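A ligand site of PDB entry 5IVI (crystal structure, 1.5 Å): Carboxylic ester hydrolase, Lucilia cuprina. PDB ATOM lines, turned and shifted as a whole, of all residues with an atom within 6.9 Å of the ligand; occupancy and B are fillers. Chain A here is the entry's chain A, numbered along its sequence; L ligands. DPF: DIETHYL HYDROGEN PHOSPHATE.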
ATOM      1  N   HIS A 141      27.663  -1.198  11.208  1.00  0.00           N
ATOM      2  CA  HIS A 141      26.680  -2.195  11.597  1.00  0.00           C
ATOM      3  C   HIS A 141      25.748  -2.498  10.439  1.00  0.00           C
ATOM      4  O   HIS A 141      25.483  -1.635   9.592  1.00  0.00           O
ATOM      5  CB  HIS A 141      25.849  -1.777  12.808  1.00  0.00           C
ATOM      6  CG  HIS A 141      24.920  -0.636  12.532  1.00  0.00           C
ATOM      7  ND1 HIS A 141      23.686  -0.794  11.921  1.00  0.00           N
ATOM      8  CD2 HIS A 141      25.046   0.689  12.784  1.00  0.00           C
ATOM      9  CE1 HIS A 141      23.106   0.376  11.808  1.00  0.00           C
ATOM     10  NE2 HIS A 141      23.905   1.302  12.335  1.00  0.00           N
ATOM     11  N   GLY A 142      25.254  -3.727  10.451  1.00  0.00           N
ATOM     12  CA  GLY A 142      24.212  -4.152   9.541  1.00  0.00           C
ATOM     13  C   GLY A 142      22.828  -3.993  10.142  1.00  0.00           C
ATOM     14  O   GLY A 142      22.634  -3.283  11.145  1.00  0.00           O
ATOM     15  N   GLY A 143      21.831  -4.598   9.515  1.00  0.00           N
ATOM     16  CA  GLY A 143      20.447  -4.315   9.852  1.00  0.00           C
ATOM     17  C   GLY A 143      19.578  -3.911   8.664  1.00  0.00           C
ATOM     18  O   GLY A 143      18.579  -3.212   8.820  1.00  0.00           O
ATOM     19  N   GLY A 144      19.952  -4.382   7.480  1.00  0.00           N
ATOM     20  CA  GLY A 144      19.162  -4.172   6.282  1.00  0.00           C
ATOM     21  C   GLY A 144      19.030  -2.722   5.848  1.00  0.00           C
ATOM     22  O   GLY A 144      18.198  -2.405   4.987  1.00  0.00           O
ATOM     23  N   PHE A 145      19.871  -1.847   6.405  1.00  0.00           N
ATOM     24  CA  PHE A 145      19.759  -0.384   6.228  1.00  0.00           C
ATOM     25  C   PHE A 145      18.470   0.143   6.841  1.00  0.00           C
ATOM     26  O   PHE A 145      18.081   1.293   6.573  1.00  0.00           O
ATOM     27  CB  PHE A 145      19.838   0.042   4.731  1.00  0.00           C
ATOM     28  CG  PHE A 145      21.129  -0.362   4.050  1.00  0.00           C
ATOM     29  CD1 PHE A 145      22.322   0.332   4.266  1.00  0.00           C
ATOM     30  CD2 PHE A 145      21.135  -1.449   3.175  1.00  0.00           C
ATOM     31  CE1 PHE A 145      23.511  -0.061   3.622  1.00  0.00           C
ATOM     32  CE2 PHE A 145      22.303  -1.846   2.551  1.00  0.00           C
ATOM     33  CZ  PHE A 145      23.493  -1.146   2.780  1.00  0.00           C
ATOM     34  N   ILE A 147      17.529  -1.075  10.466  1.00  0.00           N
ATOM     35  CA  ILE A 147      17.720  -1.088  11.921  1.00  0.00           C
ATOM     36  C   ILE A 147      19.197  -1.125  12.259  1.00  0.00           C
ATOM     37  O   ILE A 147      20.055  -1.347  11.385  1.00  0.00           O
ATOM     38  CB  ILE A 147      17.027  -2.296  12.611  1.00  0.00           C
ATOM     39  CG1 ILE A 147      17.538  -3.626  12.057  1.00  0.00           C
ATOM     40  CG2 ILE A 147      15.501  -2.193  12.477  1.00  0.00           C
ATOM     41  CD1 ILE A 147      16.977  -4.851  12.828  1.00  0.00           C
ATOM     42  N   GLU A 224      29.048  -6.441   8.913  1.00  0.00           N
ATOM     43  CA  GLU A 224      28.332  -7.686   8.650  1.00  0.00           C
ATOM     44  C   GLU A 224      27.003  -7.395   7.992  1.00  0.00           C
ATOM     45  O   GLU A 224      26.335  -6.431   8.364  1.00  0.00           O
ATOM     46  CB  GLU A 224      28.116  -8.483   9.954  1.00  0.00           C
ATOM     47  CG  GLU A 224      27.548  -9.905   9.751  1.00  0.00           C
ATOM     48  CD  GLU A 224      26.036  -9.958   9.906  1.00  0.00           C
ATOM     49  OE1 GLU A 224      25.439  -8.927  10.295  1.00  0.00           O
ATOM     50  OE2 GLU A 224      25.455 -11.024   9.641  1.00  0.00           O
ATOM     51  N   SER A 225      26.611  -8.223   7.025  1.00  0.00           N
ATOM     52  CA  SER A 225      25.355  -8.097   6.296  1.00  0.00           C
ATOM     53  C   SER A 225      25.303  -6.702   5.644  1.00  0.00           C
ATOM     54  O   SER A 225      26.174  -6.397   4.845  1.00  0.00           O
ATOM     55  CB  SER A 225      24.163  -8.365   7.222  1.00  0.00           C
ATOM     56  OG  SER A 225      22.957  -8.504   6.469  1.00  0.00           O
ATOM     57  N   ALA A 226      24.318  -5.852   5.972  1.00  0.00           N
ATOM     58  CA  ALA A 226      24.272  -4.508   5.390  1.00  0.00           C
ATOM     59  C   ALA A 226      25.505  -3.669   5.733  1.00  0.00           C
ATOM     60  O   ALA A 226      25.827  -2.731   5.033  1.00  0.00           O
ATOM     61  CB  ALA A 226      23.009  -3.759   5.836  1.00  0.00           C
ATOM     62  N   GLY A 227      26.172  -4.003   6.831  1.00  0.00           N
ATOM     63  CA  GLY A 227      27.429  -3.358   7.145  1.00  0.00           C
ATOM     64  C   GLY A 227      28.542  -3.844   6.218  1.00  0.00           C
ATOM     65  O   GLY A 227      29.512  -3.122   5.976  1.00  0.00           O
ATOM     66  N   SER A 251      29.536 -11.750   5.477  1.00  0.00           N
ATOM     67  CA  SER A 251      28.222 -12.127   4.982  1.00  0.00           C
ATOM     68  C   SER A 251      27.548 -10.981   4.248  1.00  0.00           C
ATOM     69  O   SER A 251      26.449 -10.540   4.602  1.00  0.00           O
ATOM     70  CB  SER A 251      27.327 -12.623   6.116  1.00  0.00           C
ATOM     71  OG  SER A 251      27.907 -13.738   6.785  1.00  0.00           O
ATOM     72  N   TRP A 258      19.857  -7.979  -2.215  1.00  0.00           N
ATOM     73  CA  TRP A 258      19.241  -7.154  -1.186  1.00  0.00           C
ATOM     74  C   TRP A 258      19.980  -5.845  -0.906  1.00  0.00           C
ATOM     75  O   TRP A 258      19.498  -5.025  -0.136  1.00  0.00           O
ATOM     76  CB  TRP A 258      19.142  -7.952   0.120  1.00  0.00           C
ATOM     77  CG  TRP A 258      20.434  -8.615   0.528  1.00  0.00           C
ATOM     78  CD1 TRP A 258      20.800  -9.919   0.285  1.00  0.00           C
ATOM     79  CD2 TRP A 258      21.534  -8.019   1.229  1.00  0.00           C
ATOM     80  NE1 TRP A 258      22.059 -10.164   0.814  1.00  0.00           N
ATOM     81  CE2 TRP A 258      22.528  -9.007   1.391  1.00  0.00           C
ATOM     82  CE3 TRP A 258      21.777  -6.731   1.734  1.00  0.00           C
ATOM     83  CZ2 TRP A 258      23.735  -8.768   2.032  1.00  0.00           C
ATOM     84  CZ3 TRP A 258      22.978  -6.501   2.377  1.00  0.00           C
ATOM     85  CH2 TRP A 258      23.941  -7.508   2.518  1.00  0.00           C
ATOM     86  N   ALA A 259      21.136  -5.660  -1.514  1.00  0.00           N
ATOM     87  CA  ALA A 259      22.020  -4.540  -1.130  1.00  0.00           C
ATOM     88  C   ALA A 259      21.807  -3.237  -1.872  1.00  0.00           C
ATOM     89  O   ALA A 259      22.437  -2.232  -1.548  1.00  0.00           O
ATOM     90  CB  ALA A 259      23.468  -4.974  -1.256  1.00  0.00           C
ATOM     91  N   MET A 315      13.893  -6.958  -1.037  1.00  0.00           N
ATOM     92  CA  MET A 315      13.814  -7.151   0.415  1.00  0.00           C
ATOM     93  C   MET A 315      13.390  -5.893   1.199  1.00  0.00           C
ATOM     94  O   MET A 315      12.657  -5.984   2.186  1.00  0.00           O
ATOM     95  CB  MET A 315      15.139  -7.682   0.932  1.00  0.00           C
ATOM     96  CG  MET A 315      15.000  -8.350   2.268  1.00  0.00           C
ATOM     97  SD  MET A 315      16.564  -8.941   2.923  1.00  0.00           S
ATOM     98  CE  MET A 315      16.016  -9.632   4.487  1.00  0.00           C
ATOM     99  N   PHE A 316      13.858  -4.728   0.762  1.00  0.00           N
ATOM    100  CA  PHE A 316      13.572  -3.468   1.472  1.00  0.00           C
ATOM    101  C   PHE A 316      13.084  -2.402   0.491  1.00  0.00           C
ATOM    102  O   PHE A 316      13.591  -2.338  -0.627  1.00  0.00           O
ATOM    103  CB  PHE A 316      14.815  -2.961   2.210  1.00  0.00           C
ATOM    104  CG  PHE A 316      15.517  -4.015   3.028  1.00  0.00           C
ATOM    105  CD1 PHE A 316      15.050  -4.377   4.266  1.00  0.00           C
ATOM    106  CD2 PHE A 316      16.690  -4.609   2.560  1.00  0.00           C
ATOM    107  CE1 PHE A 316      15.688  -5.344   5.033  1.00  0.00           C
ATOM    108  CE2 PHE A 316      17.344  -5.580   3.308  1.00  0.00           C
ATOM    109  CZ  PHE A 316      16.835  -5.945   4.554  1.00  0.00           C
ATOM    110  N   PHE A 361      18.858 -18.557   9.195  1.00  0.00           N
ATOM    111  CA  PHE A 361      18.110 -17.384   9.632  1.00  0.00           C
ATOM    112  C   PHE A 361      16.608 -17.313   9.353  1.00  0.00           C
ATOM    113  O   PHE A 361      15.862 -16.760  10.141  1.00  0.00           O
ATOM    114  CB  PHE A 361      18.771 -16.154   8.982  1.00  0.00           C
ATOM    115  CG  PHE A 361      18.435 -14.855   9.641  1.00  0.00           C
ATOM    116  CD1 PHE A 361      19.254 -14.348  10.649  1.00  0.00           C
ATOM    117  CD2 PHE A 361      17.315 -14.121   9.270  1.00  0.00           C
ATOM    118  CE1 PHE A 361      18.952 -13.150  11.272  1.00  0.00           C
ATOM    119  CE2 PHE A 361      17.014 -12.937   9.892  1.00  0.00           C
ATOM    120  CZ  PHE A 361      17.830 -12.444  10.889  1.00  0.00           C
ATOM    121  N   PHE A 362      16.173 -17.875   8.231  1.00  0.00           N
ATOM    122  CA  PHE A 362      14.774 -17.770   7.842  1.00  0.00           C
ATOM    123  C   PHE A 362      13.935 -18.961   8.312  1.00  0.00           C
ATOM    124  O   PHE A 362      12.864 -19.230   7.761  1.00  0.00           O
ATOM    125  CB  PHE A 362      14.647 -17.589   6.328  1.00  0.00           C
ATOM    126  CG  PHE A 362      15.553 -16.498   5.773  1.00  0.00           C
ATOM    127  CD1 PHE A 362      15.301 -15.156   6.056  1.00  0.00           C
ATOM    128  CD2 PHE A 362      16.649 -16.817   4.991  1.00  0.00           C
ATOM    129  CE1 PHE A 362      16.135 -14.162   5.559  1.00  0.00           C
ATOM    130  CE2 PHE A 362      17.476 -15.816   4.497  1.00  0.00           C
ATOM    131  CZ  PHE A 362      17.219 -14.496   4.780  1.00  0.00           C
ATOM    132  N   TYR A 427      21.300 -15.174  -1.519  1.00  0.00           N
ATOM    133  CA  TYR A 427      21.601 -13.933  -0.825  1.00  0.00           C
ATOM    134  C   TYR A 427      23.073 -13.694  -0.481  1.00  0.00           C
ATOM    135  O   TYR A 427      23.456 -12.539  -0.218  1.00  0.00           O
ATOM    136  CB  TYR A 427      20.793 -13.845   0.477  1.00  0.00           C
ATOM    137  CG  TYR A 427      19.295 -13.690   0.281  1.00  0.00           C
ATOM    138  CD1 TYR A 427      18.761 -12.581  -0.377  1.00  0.00           C
ATOM    139  CD2 TYR A 427      18.414 -14.655   0.747  1.00  0.00           C
ATOM    140  CE1 TYR A 427      17.393 -12.443  -0.546  1.00  0.00           C
ATOM    141  CE2 TYR A 427      17.044 -14.530   0.567  1.00  0.00           C
ATOM    142  CZ  TYR A 427      16.551 -13.421  -0.065  1.00  0.00           C
ATOM    143  OH  TYR A 427      15.186 -13.293  -0.215  1.00  0.00           O
ATOM    144  N   PHE A 428      23.896 -14.735  -0.489  1.00  0.00           N
ATOM    145  CA  PHE A 428      25.270 -14.598   0.011  1.00  0.00           C
ATOM    146  C   PHE A 428      26.364 -15.258  -0.845  1.00  0.00           C
ATOM    147  O   PHE A 428      27.263 -14.569  -1.324  1.00  0.00           O
ATOM    148  CB  PHE A 428      25.340 -15.116   1.453  1.00  0.00           C
ATOM    149  CG  PHE A 428      24.405 -14.392   2.387  1.00  0.00           C
ATOM    150  CD1 PHE A 428      24.696 -13.107   2.826  1.00  0.00           C
ATOM    151  CD2 PHE A 428      23.232 -14.994   2.833  1.00  0.00           C
ATOM    152  CE1 PHE A 428      23.804 -12.427   3.670  1.00  0.00           C
ATOM    153  CE2 PHE A 428      22.369 -14.334   3.684  1.00  0.00           C
ATOM    154  CZ  PHE A 428      22.648 -13.047   4.095  1.00  0.00           C
ATOM    155  N   TYR A 464      20.146 -10.890  17.729  1.00  0.00           N
ATOM    156  CA  TYR A 464      19.533 -11.275  16.463  1.00  0.00           C
ATOM    157  C   TYR A 464      18.885 -12.650  16.598  1.00  0.00           C
ATOM    158  O   TYR A 464      17.921 -12.937  15.897  1.00  0.00           O
ATOM    159  CB  TYR A 464      20.549 -11.309  15.346  1.00  0.00           C
ATOM    160  CG  TYR A 464      20.872  -9.994  14.658  1.00  0.00           C
ATOM    161  CD1 TYR A 464      19.927  -9.350  13.869  1.00  0.00           C
ATOM    162  CD2 TYR A 464      22.147  -9.455  14.723  1.00  0.00           C
ATOM    163  CE1 TYR A 464      20.237  -8.183  13.219  1.00  0.00           C
ATOM    164  CE2 TYR A 464      22.472  -8.292  14.054  1.00  0.00           C
ATOM    165  CZ  TYR A 464      21.508  -7.661  13.305  1.00  0.00           C
ATOM    166  OH  TYR A 464      21.830  -6.493  12.649  1.00  0.00           O
ATOM    167  N   MET A 467      15.489 -11.901  17.883  1.00  0.00           N
ATOM    168  CA  MET A 467      14.734 -11.303  16.793  1.00  0.00           C
ATOM    169  C   MET A 467      14.164 -12.336  15.844  1.00  0.00           C
ATOM    170  O   MET A 467      13.029 -12.193  15.393  1.00  0.00           O
ATOM    171  CB  MET A 467      15.606 -10.341  15.989  1.00  0.00           C
ATOM    172  CG  MET A 467      14.844  -9.542  14.954  1.00  0.00           C
ATOM    173  SD  MET A 467      15.957  -8.642  13.836  1.00  0.00           S
ATOM    174  CE  MET A 467      16.637 -10.013  12.936  1.00  0.00           C
ATOM    175  N   HIS A 478      23.090 -16.862   9.607  1.00  0.00           N
ATOM    176  CA  HIS A 478      23.353 -15.442   9.441  1.00  0.00           C
ATOM    177  C   HIS A 478      23.267 -14.724  10.793  1.00  0.00           C
ATOM    178  O   HIS A 478      22.278 -14.887  11.537  1.00  0.00           O
ATOM    179  CB  HIS A 478      22.352 -14.829   8.465  1.00  0.00           C
ATOM    180  CG  HIS A 478      22.693 -13.437   8.031  1.00  0.00           C
ATOM    181  ND1 HIS A 478      23.848 -13.142   7.344  1.00  0.00           N
ATOM    182  CD2 HIS A 478      22.019 -12.272   8.158  1.00  0.00           C
ATOM    183  CE1 HIS A 478      23.884 -11.845   7.073  1.00  0.00           C
ATOM    184  NE2 HIS A 478      22.774 -11.298   7.551  1.00  0.00           N
ATOM    185  N   THR A 479      24.314 -13.939  11.072  1.00  0.00           N
ATOM    186  CA  THR A 479      24.545 -13.129  12.288  1.00  0.00           C
ATOM    187  C   THR A 479      25.109 -13.901  13.481  1.00  0.00           C
ATOM    188  O   THR A 479      25.379 -13.287  14.507  1.00  0.00           O
ATOM    189  CB  THR A 479      23.284 -12.375  12.811  1.00  0.00           C
ATOM    190  OG1 THR A 479      22.407 -13.297  13.456  1.00  0.00           O
ATOM    191  CG2 THR A 479      22.550 -11.635  11.681  1.00  0.00           C
ATOM    192  N   LEU A 482      28.651 -12.767  15.137  1.00  0.00           N
ATOM    193  CA  LEU A 482      28.811 -11.466  15.791  1.00  0.00           C
ATOM    194  C   LEU A 482      29.026 -11.590  17.292  1.00  0.00           C
ATOM    195  O   LEU A 482      29.760 -10.798  17.902  1.00  0.00           O
ATOM    196  CB  LEU A 482      27.594 -10.584  15.501  1.00  0.00           C
ATOM    197  CG  LEU A 482      27.540 -10.120  14.047  1.00  0.00           C
ATOM    198  CD1 LEU A 482      26.282  -9.342  13.831  1.00  0.00           C
ATOM    199  CD2 LEU A 482      28.763  -9.276  13.688  1.00  0.00           C
HETATM  200  O4  DPF L   1      21.817  -6.450   7.332  1.00  0.00           O
HETATM  201  P1  DPF L   1      21.617  -7.884   6.938  1.00  0.00           P
HETATM  202  O3  DPF L   1      20.757  -8.013   5.620  1.00  0.00           O
HETATM  203  C1  DPF L   1      20.747  -9.311   5.075  1.00  0.00           C
HETATM  204  C4  DPF L   1      19.829  -9.425   3.894  1.00  0.00           C
HETATM  205  O1  DPF L   1      20.816  -8.623   8.062  1.00  0.00           O
HETATM  206  C2  DPF L   1      21.286  -8.631   9.380  1.00  0.00           C
HETATM  207  C3  DPF L   1      20.233  -9.418  10.118  1.00  0.00           C
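C of Gly 142 touches O4 of the ligand, at 3.9 Å. CD2 of Trp 258 touches C4 of the ligand (3.5 Å). Met 315 touches the ligand (SD to C4, 3.4 Å). Phe 361 touches the ligand (CZ to C3, 3.9 Å). Tyr 464 touches the ligand (CE1 to C3, 3.3 Å). Thr 479 touches the ligand. Hydrophobic or aromatic side chains that line the ligand: Ala 226, Trp 258, Met 315, Phe 361, Tyr 464 and His 478. 11 residues have an atom within 4 Å of the ligand: Gly 142, Gly 143, Gly 144, Ser 225, Ala 226, Trp 258, Met 315, Phe 361, Tyr 464, His 478 and Thr 479.
The indole nitrogen (NE1) of Trp 258 lies within hydrogen-bond range of the backbone carbonyl oxygen (O) of Tyr 427 (2.9 Å). The side-chain carboxylate (OE2) of Glu 224 lies close to a ring nitrogen (NE2) of His 478, 3.4 Å away. The backbone NH (N) of Ser 225 lies close to the backbone carbonyl oxygen (O) of Ser 251 (3.4 Å). The side-chain carboxylate of Glu 224 lies within hydrogen-bond range of the backbone NH of Thr 479, 3.4 Å away. A ring nitrogen (NE2) of His 478 is in hydrogen-bond range of the side-chain hydroxyl (OG) of Ser 225, at 3.0 Å.
The backbone NH (N) of Ala 226 is in hydrogen-bond range of an oxygen (O4) of the ligand (2.9 Å). O4 of the ligand is in hydrogen-bond range of N of Gly 144, at 2.8 Å. O1 of the ligand is in hydrogen-bond range of NE2 of His 478 (3.4 Å). P1 of the ligand is bonded to OG of Ser 225 (1.5 Å). The backbone NH of Gly 143 sits at hydrogen-bond distance from an oxygen (O4) of the ligand (2.9 Å).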
